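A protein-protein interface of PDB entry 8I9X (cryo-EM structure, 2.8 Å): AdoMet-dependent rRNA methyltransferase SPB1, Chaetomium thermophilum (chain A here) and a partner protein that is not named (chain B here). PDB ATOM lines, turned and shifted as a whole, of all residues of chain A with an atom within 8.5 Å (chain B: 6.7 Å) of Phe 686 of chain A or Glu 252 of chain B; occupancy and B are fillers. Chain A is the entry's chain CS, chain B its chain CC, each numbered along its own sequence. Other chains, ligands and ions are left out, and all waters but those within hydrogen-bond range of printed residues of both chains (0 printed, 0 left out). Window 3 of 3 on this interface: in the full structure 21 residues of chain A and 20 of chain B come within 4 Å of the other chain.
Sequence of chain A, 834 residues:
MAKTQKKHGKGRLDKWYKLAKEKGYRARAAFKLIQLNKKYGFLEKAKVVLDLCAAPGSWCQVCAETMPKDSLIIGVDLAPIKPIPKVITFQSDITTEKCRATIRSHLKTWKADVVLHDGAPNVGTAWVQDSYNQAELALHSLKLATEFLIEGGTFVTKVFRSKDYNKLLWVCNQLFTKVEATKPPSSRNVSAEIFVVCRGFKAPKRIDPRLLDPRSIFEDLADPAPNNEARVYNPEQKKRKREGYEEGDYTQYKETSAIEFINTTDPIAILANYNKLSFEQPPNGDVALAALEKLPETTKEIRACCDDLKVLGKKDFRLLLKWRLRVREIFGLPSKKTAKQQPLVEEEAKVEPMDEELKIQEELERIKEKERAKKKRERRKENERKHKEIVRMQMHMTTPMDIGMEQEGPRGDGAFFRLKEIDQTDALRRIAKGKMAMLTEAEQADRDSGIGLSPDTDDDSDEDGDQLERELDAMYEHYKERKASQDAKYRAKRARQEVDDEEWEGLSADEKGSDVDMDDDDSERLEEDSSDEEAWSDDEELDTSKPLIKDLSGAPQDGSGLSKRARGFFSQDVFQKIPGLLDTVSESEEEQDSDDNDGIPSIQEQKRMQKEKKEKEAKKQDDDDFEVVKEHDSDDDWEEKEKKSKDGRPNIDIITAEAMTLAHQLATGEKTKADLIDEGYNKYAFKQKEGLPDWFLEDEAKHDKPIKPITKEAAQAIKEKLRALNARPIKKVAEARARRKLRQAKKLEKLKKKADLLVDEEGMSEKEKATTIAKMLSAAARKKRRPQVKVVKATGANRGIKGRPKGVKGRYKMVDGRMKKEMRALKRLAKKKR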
ATOM      1  N   GLY A 680      15.370  -4.820  19.205  1.00  0.00           N
ATOM      2  CA  GLY A 680      16.636  -4.767  19.910  1.00  0.00           C
ATOM      3  C   GLY A 680      17.594  -5.854  19.479  1.00  0.00           C
ATOM      4  O   GLY A 680      18.811  -5.703  19.622  1.00  0.00           O
ATOM      5  N   TYR A 681      17.073  -6.960  18.955  1.00  0.00           N
ATOM      6  CA  TYR A 681      17.947  -7.947  18.315  1.00  0.00           C
ATOM      7  C   TYR A 681      18.263  -7.499  16.885  1.00  0.00           C
ATOM      8  O   TYR A 681      17.778  -8.044  15.893  1.00  0.00           O
ATOM      9  CB  TYR A 681      17.332  -9.339  18.352  1.00  0.00           C
ATOM     10  CG  TYR A 681      17.438 -10.039  19.692  1.00  0.00           C
ATOM     11  CD1 TYR A 681      17.817  -9.358  20.837  1.00  0.00           C
ATOM     12  CD2 TYR A 681      17.207 -11.399  19.797  1.00  0.00           C
ATOM     13  CE1 TYR A 681      17.922 -10.013  22.052  1.00  0.00           C
ATOM     14  CE2 TYR A 681      17.311 -12.058  21.001  1.00  0.00           C
ATOM     15  CZ  TYR A 681      17.668 -11.363  22.125  1.00  0.00           C
ATOM     16  OH  TYR A 681      17.776 -12.023  23.327  1.00  0.00           O
ATOM     17  N   ASN A 682      19.101  -6.469  16.802  1.00  0.00           N
ATOM     18  CA  ASN A 682      19.550  -5.890  15.546  1.00  0.00           C
ATOM     19  C   ASN A 682      21.040  -6.170  15.343  1.00  0.00           C
ATOM     20  O   ASN A 682      21.664  -6.922  16.095  1.00  0.00           O
ATOM     21  CB  ASN A 682      19.244  -4.392  15.519  1.00  0.00           C
ATOM     22  CG  ASN A 682      19.715  -3.673  16.769  1.00  0.00           C
ATOM     23  OD1 ASN A 682      20.645  -4.114  17.442  1.00  0.00           O
ATOM     24  ND2 ASN A 682      19.072  -2.556  17.082  1.00  0.00           N
ATOM     25  N   LYS A 683      21.622  -5.556  14.308  1.00  0.00           N
ATOM     26  CA  LYS A 683      23.035  -5.756  14.007  1.00  0.00           C
ATOM     27  C   LYS A 683      23.957  -5.206  15.088  1.00  0.00           C
ATOM     28  O   LYS A 683      25.093  -5.674  15.208  1.00  0.00           O
ATOM     29  CB  LYS A 683      23.382  -5.120  12.661  1.00  0.00           C
ATOM     30  CG  LYS A 683      23.256  -3.610  12.631  1.00  0.00           C
ATOM     31  CD  LYS A 683      23.573  -3.065  11.250  1.00  0.00           C
ATOM     32  CE  LYS A 683      23.466  -1.553  11.212  1.00  0.00           C
ATOM     33  NZ  LYS A 683      23.769  -1.013   9.859  1.00  0.00           N
ATOM     34  N   TYR A 684      23.506  -4.227  15.870  1.00  0.00           N
ATOM     35  CA  TYR A 684      24.318  -3.701  16.958  1.00  0.00           C
ATOM     36  C   TYR A 684      24.293  -4.582  18.198  1.00  0.00           C
ATOM     37  O   TYR A 684      25.064  -4.333  19.129  1.00  0.00           O
ATOM     38  CB  TYR A 684      23.861  -2.291  17.329  1.00  0.00           C
ATOM     39  CG  TYR A 684      23.907  -1.310  16.183  1.00  0.00           C
ATOM     40  CD1 TYR A 684      25.085  -0.660  15.852  1.00  0.00           C
ATOM     41  CD2 TYR A 684      22.774  -1.029  15.437  1.00  0.00           C
ATOM     42  CE1 TYR A 684      25.137   0.238  14.810  1.00  0.00           C
ATOM     43  CE2 TYR A 684      22.815  -0.133  14.391  1.00  0.00           C
ATOM     44  CZ  TYR A 684      23.999   0.498  14.082  1.00  0.00           C
ATOM     45  OH  TYR A 684      24.046   1.394  13.040  1.00  0.00           O
ATOM     46  N   ALA A 685      23.435  -5.595  18.233  1.00  0.00           N
ATOM     47  CA  ALA A 685      23.347  -6.464  19.392  1.00  0.00           C
ATOM     48  C   ALA A 685      24.524  -7.435  19.429  1.00  0.00           C
ATOM     49  O   ALA A 685      25.201  -7.674  18.426  1.00  0.00           O
ATOM     50  CB  ALA A 685      22.029  -7.235  19.385  1.00  0.00           C
ATOM     51  N   PHE A 686      24.759  -7.995  20.616  1.00  0.00           N
ATOM     52  CA  PHE A 686      25.812  -8.987  20.834  1.00  0.00           C
ATOM     53  C   PHE A 686      27.184  -8.446  20.441  1.00  0.00           C
ATOM     54  O   PHE A 686      28.013  -9.155  19.868  1.00  0.00           O
ATOM     55  CB  PHE A 686      25.510 -10.290  20.093  1.00  0.00           C
ATOM     56  CG  PHE A 686      24.165 -10.870  20.414  1.00  0.00           C
ATOM     57  CD1 PHE A 686      23.147 -10.858  19.480  1.00  0.00           C
ATOM     58  CD2 PHE A 686      23.923 -11.434  21.652  1.00  0.00           C
ATOM     59  CE1 PHE A 686      21.911 -11.396  19.777  1.00  0.00           C
ATOM     60  CE2 PHE A 686      22.691 -11.972  21.954  1.00  0.00           C
ATOM     61  CZ  PHE A 686      21.684 -11.953  21.017  1.00  0.00           C
ATOM     62  N   LYS A 687      27.428  -7.178  20.755  1.00  0.00           N
ATOM     63  CA  LYS A 687      28.705  -6.536  20.487  1.00  0.00           C
ATOM     64  C   LYS A 687      29.461  -6.367  21.798  1.00  0.00           C
ATOM     65  O   LYS A 687      28.908  -5.859  22.778  1.00  0.00           O
ATOM     66  CB  LYS A 687      28.493  -5.187  19.799  1.00  0.00           C
ATOM     67  CG  LYS A 687      29.767  -4.505  19.366  1.00  0.00           C
ATOM     68  CD  LYS A 687      29.485  -3.150  18.749  1.00  0.00           C
ATOM     69  CE  LYS A 687      28.885  -3.304  17.363  1.00  0.00           C
ATOM     70  NZ  LYS A 687      28.707  -1.990  16.689  1.00  0.00           N
ATOM     71  N   GLN A 688      30.719  -6.802  21.814  1.00  0.00           N
ATOM     72  CA  GLN A 688      31.478  -6.851  23.055  1.00  0.00           C
ATOM     73  C   GLN A 688      31.825  -5.448  23.544  1.00  0.00           C
ATOM     74  O   GLN A 688      32.074  -4.538  22.750  1.00  0.00           O
ATOM     75  CB  GLN A 688      32.752  -7.672  22.858  1.00  0.00           C
ATOM     76  CG  GLN A 688      33.617  -7.805  24.097  1.00  0.00           C
ATOM     77  CD  GLN A 688      34.975  -8.400  23.800  1.00  0.00           C
ATOM     78  OE1 GLN A 688      35.078  -9.437  23.152  1.00  0.00           O
ATOM     79  NE2 GLN A 688      36.024  -7.754  24.287  1.00  0.00           N
ATOM     80  N   LYS A 689      31.825  -5.279  24.865  1.00  0.00           N
ATOM     81  CA  LYS A 689      32.251  -4.041  25.506  1.00  0.00           C
ATOM     82  C   LYS A 689      33.187  -4.244  26.689  1.00  0.00           C
ATOM     83  O   LYS A 689      33.789  -3.264  27.143  1.00  0.00           O
ATOM     84  CB  LYS A 689      31.036  -3.234  25.990  1.00  0.00           C
ATOM     85  CG  LYS A 689      30.060  -2.816  24.906  1.00  0.00           C
ATOM     86  CD  LYS A 689      30.686  -1.834  23.936  1.00  0.00           C
ATOM     87  CE  LYS A 689      29.651  -1.297  22.962  1.00  0.00           C
ATOM     88  NZ  LYS A 689      29.179  -2.342  22.014  1.00  0.00           N
ATOM     89  N   GLY B 245      22.149  -1.901  24.222  1.00  0.00           N
ATOM     90  CA  GLY B 245      22.319  -3.092  23.421  1.00  0.00           C
ATOM     91  C   GLY B 245      23.031  -4.243  24.094  1.00  0.00           C
ATOM     92  O   GLY B 245      23.178  -5.303  23.471  1.00  0.00           O
ATOM     93  N   LEU B 246      23.477  -4.082  25.342  1.00  0.00           N
ATOM     94  CA  LEU B 246      24.311  -5.106  25.965  1.00  0.00           C
ATOM     95  C   LEU B 246      23.536  -6.400  26.202  1.00  0.00           C
ATOM     96  O   LEU B 246      23.997  -7.481  25.819  1.00  0.00           O
ATOM     97  CB  LEU B 246      24.915  -4.574  27.271  1.00  0.00           C
ATOM     98  CG  LEU B 246      24.077  -4.369  28.539  1.00  0.00           C
ATOM     99  CD1 LEU B 246      24.980  -4.202  29.752  1.00  0.00           C
ATOM    100  CD2 LEU B 246      23.134  -3.180  28.408  1.00  0.00           C
ATOM    101  N   ILE B 247      22.366  -6.317  26.828  1.00  0.00           N
ATOM    102  CA  ILE B 247      21.549  -7.494  27.122  1.00  0.00           C
ATOM    103  C   ILE B 247      20.098  -7.171  26.786  1.00  0.00           C
ATOM    104  O   ILE B 247      19.328  -6.801  27.684  1.00  0.00           O
ATOM    105  CB  ILE B 247      21.693  -7.935  28.589  1.00  0.00           C
ATOM    106  CG1 ILE B 247      23.165  -8.097  28.974  1.00  0.00           C
ATOM    107  CG2 ILE B 247      20.966  -9.250  28.825  1.00  0.00           C
ATOM    108  CD1 ILE B 247      23.384  -8.386  30.443  1.00  0.00           C
ATOM    109  N   PRO B 248      19.684  -7.268  25.520  1.00  0.00           N
ATOM    110  CA  PRO B 248      18.288  -6.942  25.189  1.00  0.00           C
ATOM    111  C   PRO B 248      17.277  -7.861  25.859  1.00  0.00           C
ATOM    112  O   PRO B 248      16.165  -7.414  26.165  1.00  0.00           O
ATOM    113  CB  PRO B 248      18.247  -7.068  23.659  1.00  0.00           C
ATOM    114  CG  PRO B 248      19.695  -7.130  23.222  1.00  0.00           C
ATOM    115  CD  PRO B 248      20.413  -7.783  24.352  1.00  0.00           C
ATOM    116  N   ASP B 249      17.625  -9.125  26.095  1.00  0.00           N
ATOM    117  CA  ASP B 249      16.740 -10.061  26.772  1.00  0.00           C
ATOM    118  C   ASP B 249      17.543 -10.882  27.770  1.00  0.00           C
ATOM    119  O   ASP B 249      18.721 -11.177  27.551  1.00  0.00           O
ATOM    120  CB  ASP B 249      16.024 -10.988  25.780  1.00  0.00           C
ATOM    121  CG  ASP B 249      14.768 -11.605  26.361  1.00  0.00           C
ATOM    122  OD1 ASP B 249      14.370 -11.208  27.477  1.00  0.00           O
ATOM    123  OD2 ASP B 249      14.177 -12.489  25.704  1.00  0.00           O
ATOM    124  N   ASP B 250      16.889 -11.255  28.866  1.00  0.00           N
ATOM    125  CA  ASP B 250      17.559 -11.949  29.955  1.00  0.00           C
ATOM    126  C   ASP B 250      17.627 -13.452  29.693  1.00  0.00           C
ATOM    127  O   ASP B 250      16.967 -13.986  28.796  1.00  0.00           O
ATOM    128  CB  ASP B 250      16.840 -11.684  31.278  1.00  0.00           C
ATOM    129  CG  ASP B 250      16.624 -10.207  31.539  1.00  0.00           C
ATOM    130  OD1 ASP B 250      17.448  -9.392  31.073  1.00  0.00           O
ATOM    131  OD2 ASP B 250      15.627  -9.860  32.208  1.00  0.00           O
ATOM    132  N   VAL B 251      18.447 -14.128  30.502  1.00  0.00           N
ATOM    133  CA  VAL B 251      18.615 -15.580  30.471  1.00  0.00           C
ATOM    134  C   VAL B 251      19.079 -15.998  29.079  1.00  0.00           C
ATOM    135  O   VAL B 251      18.284 -16.464  28.255  1.00  0.00           O
ATOM    136  CB  VAL B 251      17.318 -16.304  30.889  1.00  0.00           C
ATOM    137  CG1 VAL B 251      17.479 -17.822  30.798  1.00  0.00           C
ATOM    138  CG2 VAL B 251      16.909 -15.888  32.293  1.00  0.00           C
ATOM    139  N   GLU B 252      20.363 -15.791  28.796  1.00  0.00           N
ATOM    140  CA  GLU B 252      20.925 -16.144  27.501  1.00  0.00           C
ATOM    141  C   GLU B 252      22.436 -16.265  27.623  1.00  0.00           C
ATOM    142  O   GLU B 252      23.045 -15.767  28.574  1.00  0.00           O
ATOM    143  CB  GLU B 252      20.548 -15.112  26.430  1.00  0.00           C
ATOM    144  CG  GLU B 252      21.006 -13.697  26.743  1.00  0.00           C
ATOM    145  CD  GLU B 252      22.299 -13.335  26.045  1.00  0.00           C
ATOM    146  OE1 GLU B 252      22.648 -14.005  25.050  1.00  0.00           O
ATOM    147  OE2 GLU B 252      22.971 -12.381  26.493  1.00  0.00           O
ATOM    148  N   ASP B 253      23.034 -16.940  26.643  1.00  0.00           N
ATOM    149  CA  ASP B 253      24.484 -17.065  26.571  1.00  0.00           C
ATOM    150  C   ASP B 253      25.007 -16.173  25.456  1.00  0.00           C
ATOM    151  O   ASP B 253      24.753 -16.463  24.278  1.00  0.00           O
ATOM    152  CB  ASP B 253      24.887 -18.508  26.315  1.00  0.00           C
ATOM    153  CG  ASP B 253      26.384 -18.730  26.433  1.00  0.00           C
ATOM    154  OD1 ASP B 253      27.123 -17.758  26.689  1.00  0.00           O
ATOM    155  OD2 ASP B 253      26.824 -19.887  26.266  1.00  0.00           O
ATOM    156  N   PRO B 254      25.721 -15.090  25.768  1.00  0.00           N
ATOM    157  CA  PRO B 254      26.205 -14.206  24.697  1.00  0.00           C
ATOM    158  C   PRO B 254      27.169 -14.886  23.745  1.00  0.00           C
ATOM    159  O   PRO B 254      27.219 -14.517  22.566  1.00  0.00           O
ATOM    160  CB  PRO B 254      26.883 -13.060  25.467  1.00  0.00           C
ATOM    161  CG  PRO B 254      26.379 -13.179  26.879  1.00  0.00           C
ATOM    162  CD  PRO B 254      26.161 -14.639  27.095  1.00  0.00           C
ATOM    163  N   TYR B 255      27.931 -15.871  24.217  1.00  0.00           N
ATOM    164  CA  TYR B 255      28.983 -16.514  23.431  1.00  0.00           C
ATOM    165  C   TYR B 255      28.770 -18.019  23.485  1.00  0.00           C
ATOM    166  O   TYR B 255      29.473 -18.734  24.210  1.00  0.00           O
ATOM    167  CB  TYR B 255      30.367 -16.135  23.959  1.00  0.00           C
ATOM    168  CG  TYR B 255      30.573 -14.647  24.097  1.00  0.00           C
ATOM    169  CD1 TYR B 255      30.808 -13.851  22.987  1.00  0.00           C
ATOM    170  CD2 TYR B 255      30.523 -14.037  25.339  1.00  0.00           C
ATOM    171  CE1 TYR B 255      30.995 -12.492  23.113  1.00  0.00           C
ATOM    172  CE2 TYR B 255      30.708 -12.679  25.474  1.00  0.00           C
ATOM    173  CZ  TYR B 255      30.943 -11.912  24.358  1.00  0.00           C
ATOM    174  OH  TYR B 255      31.127 -10.556  24.488  1.00  0.00           O
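O of Gly 680 of chain A sits close to OD1 of Asn 682 of chain A, 3.3 Å away. N of Tyr 255 of chain B sits close to OD1 of Asp 253 of chain B (3.2 Å).
Hydrophobic or aromatic side chains of chain B within 4 Å of the printed part of chain A: Pro 248 and Tyr 255. Of the 10 printed residues of chain A, 4 touch a printed residue of chain B. Hydrophobic or aromatic side chains of chain A within 4 Å of the printed part of chain B: Tyr 681 and Phe 686. Among the printed residues, 5 pairs touch across the chains.
Among the printed residues, pairs that only touch across the chains: Gly 680 of chain A with Pro 248 of chain B, Tyr 681 of chain A with Pro 248 of chain B, Tyr 681 of chain A with Asp 249 of chain B, Phe 686 of chain A with Glu 252 of chain B and Gln 688 of chain A with Tyr 255 of chain B.
Printed residues of chain B within 4 Å of Phe 686 of chain A: Glu 252. Glu 252 of chain B touches one residue of chain A. Of the printed residues of chain B, Gly 680 of chain A touches Pro 248. Of the printed residues of chain A, Asp 249 of chain B touches Tyr 681. Asn 682 of chain A touches none of the printed residues of chain B. The nearest residue of chain A that does not touch Glu 252 of chain B is Tyr 681 of chain A (5.0 Å). The nearest printed residue of chain A that does not touch Pro 248 of chain B is Ala 685 of chain A (4.5 Å).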
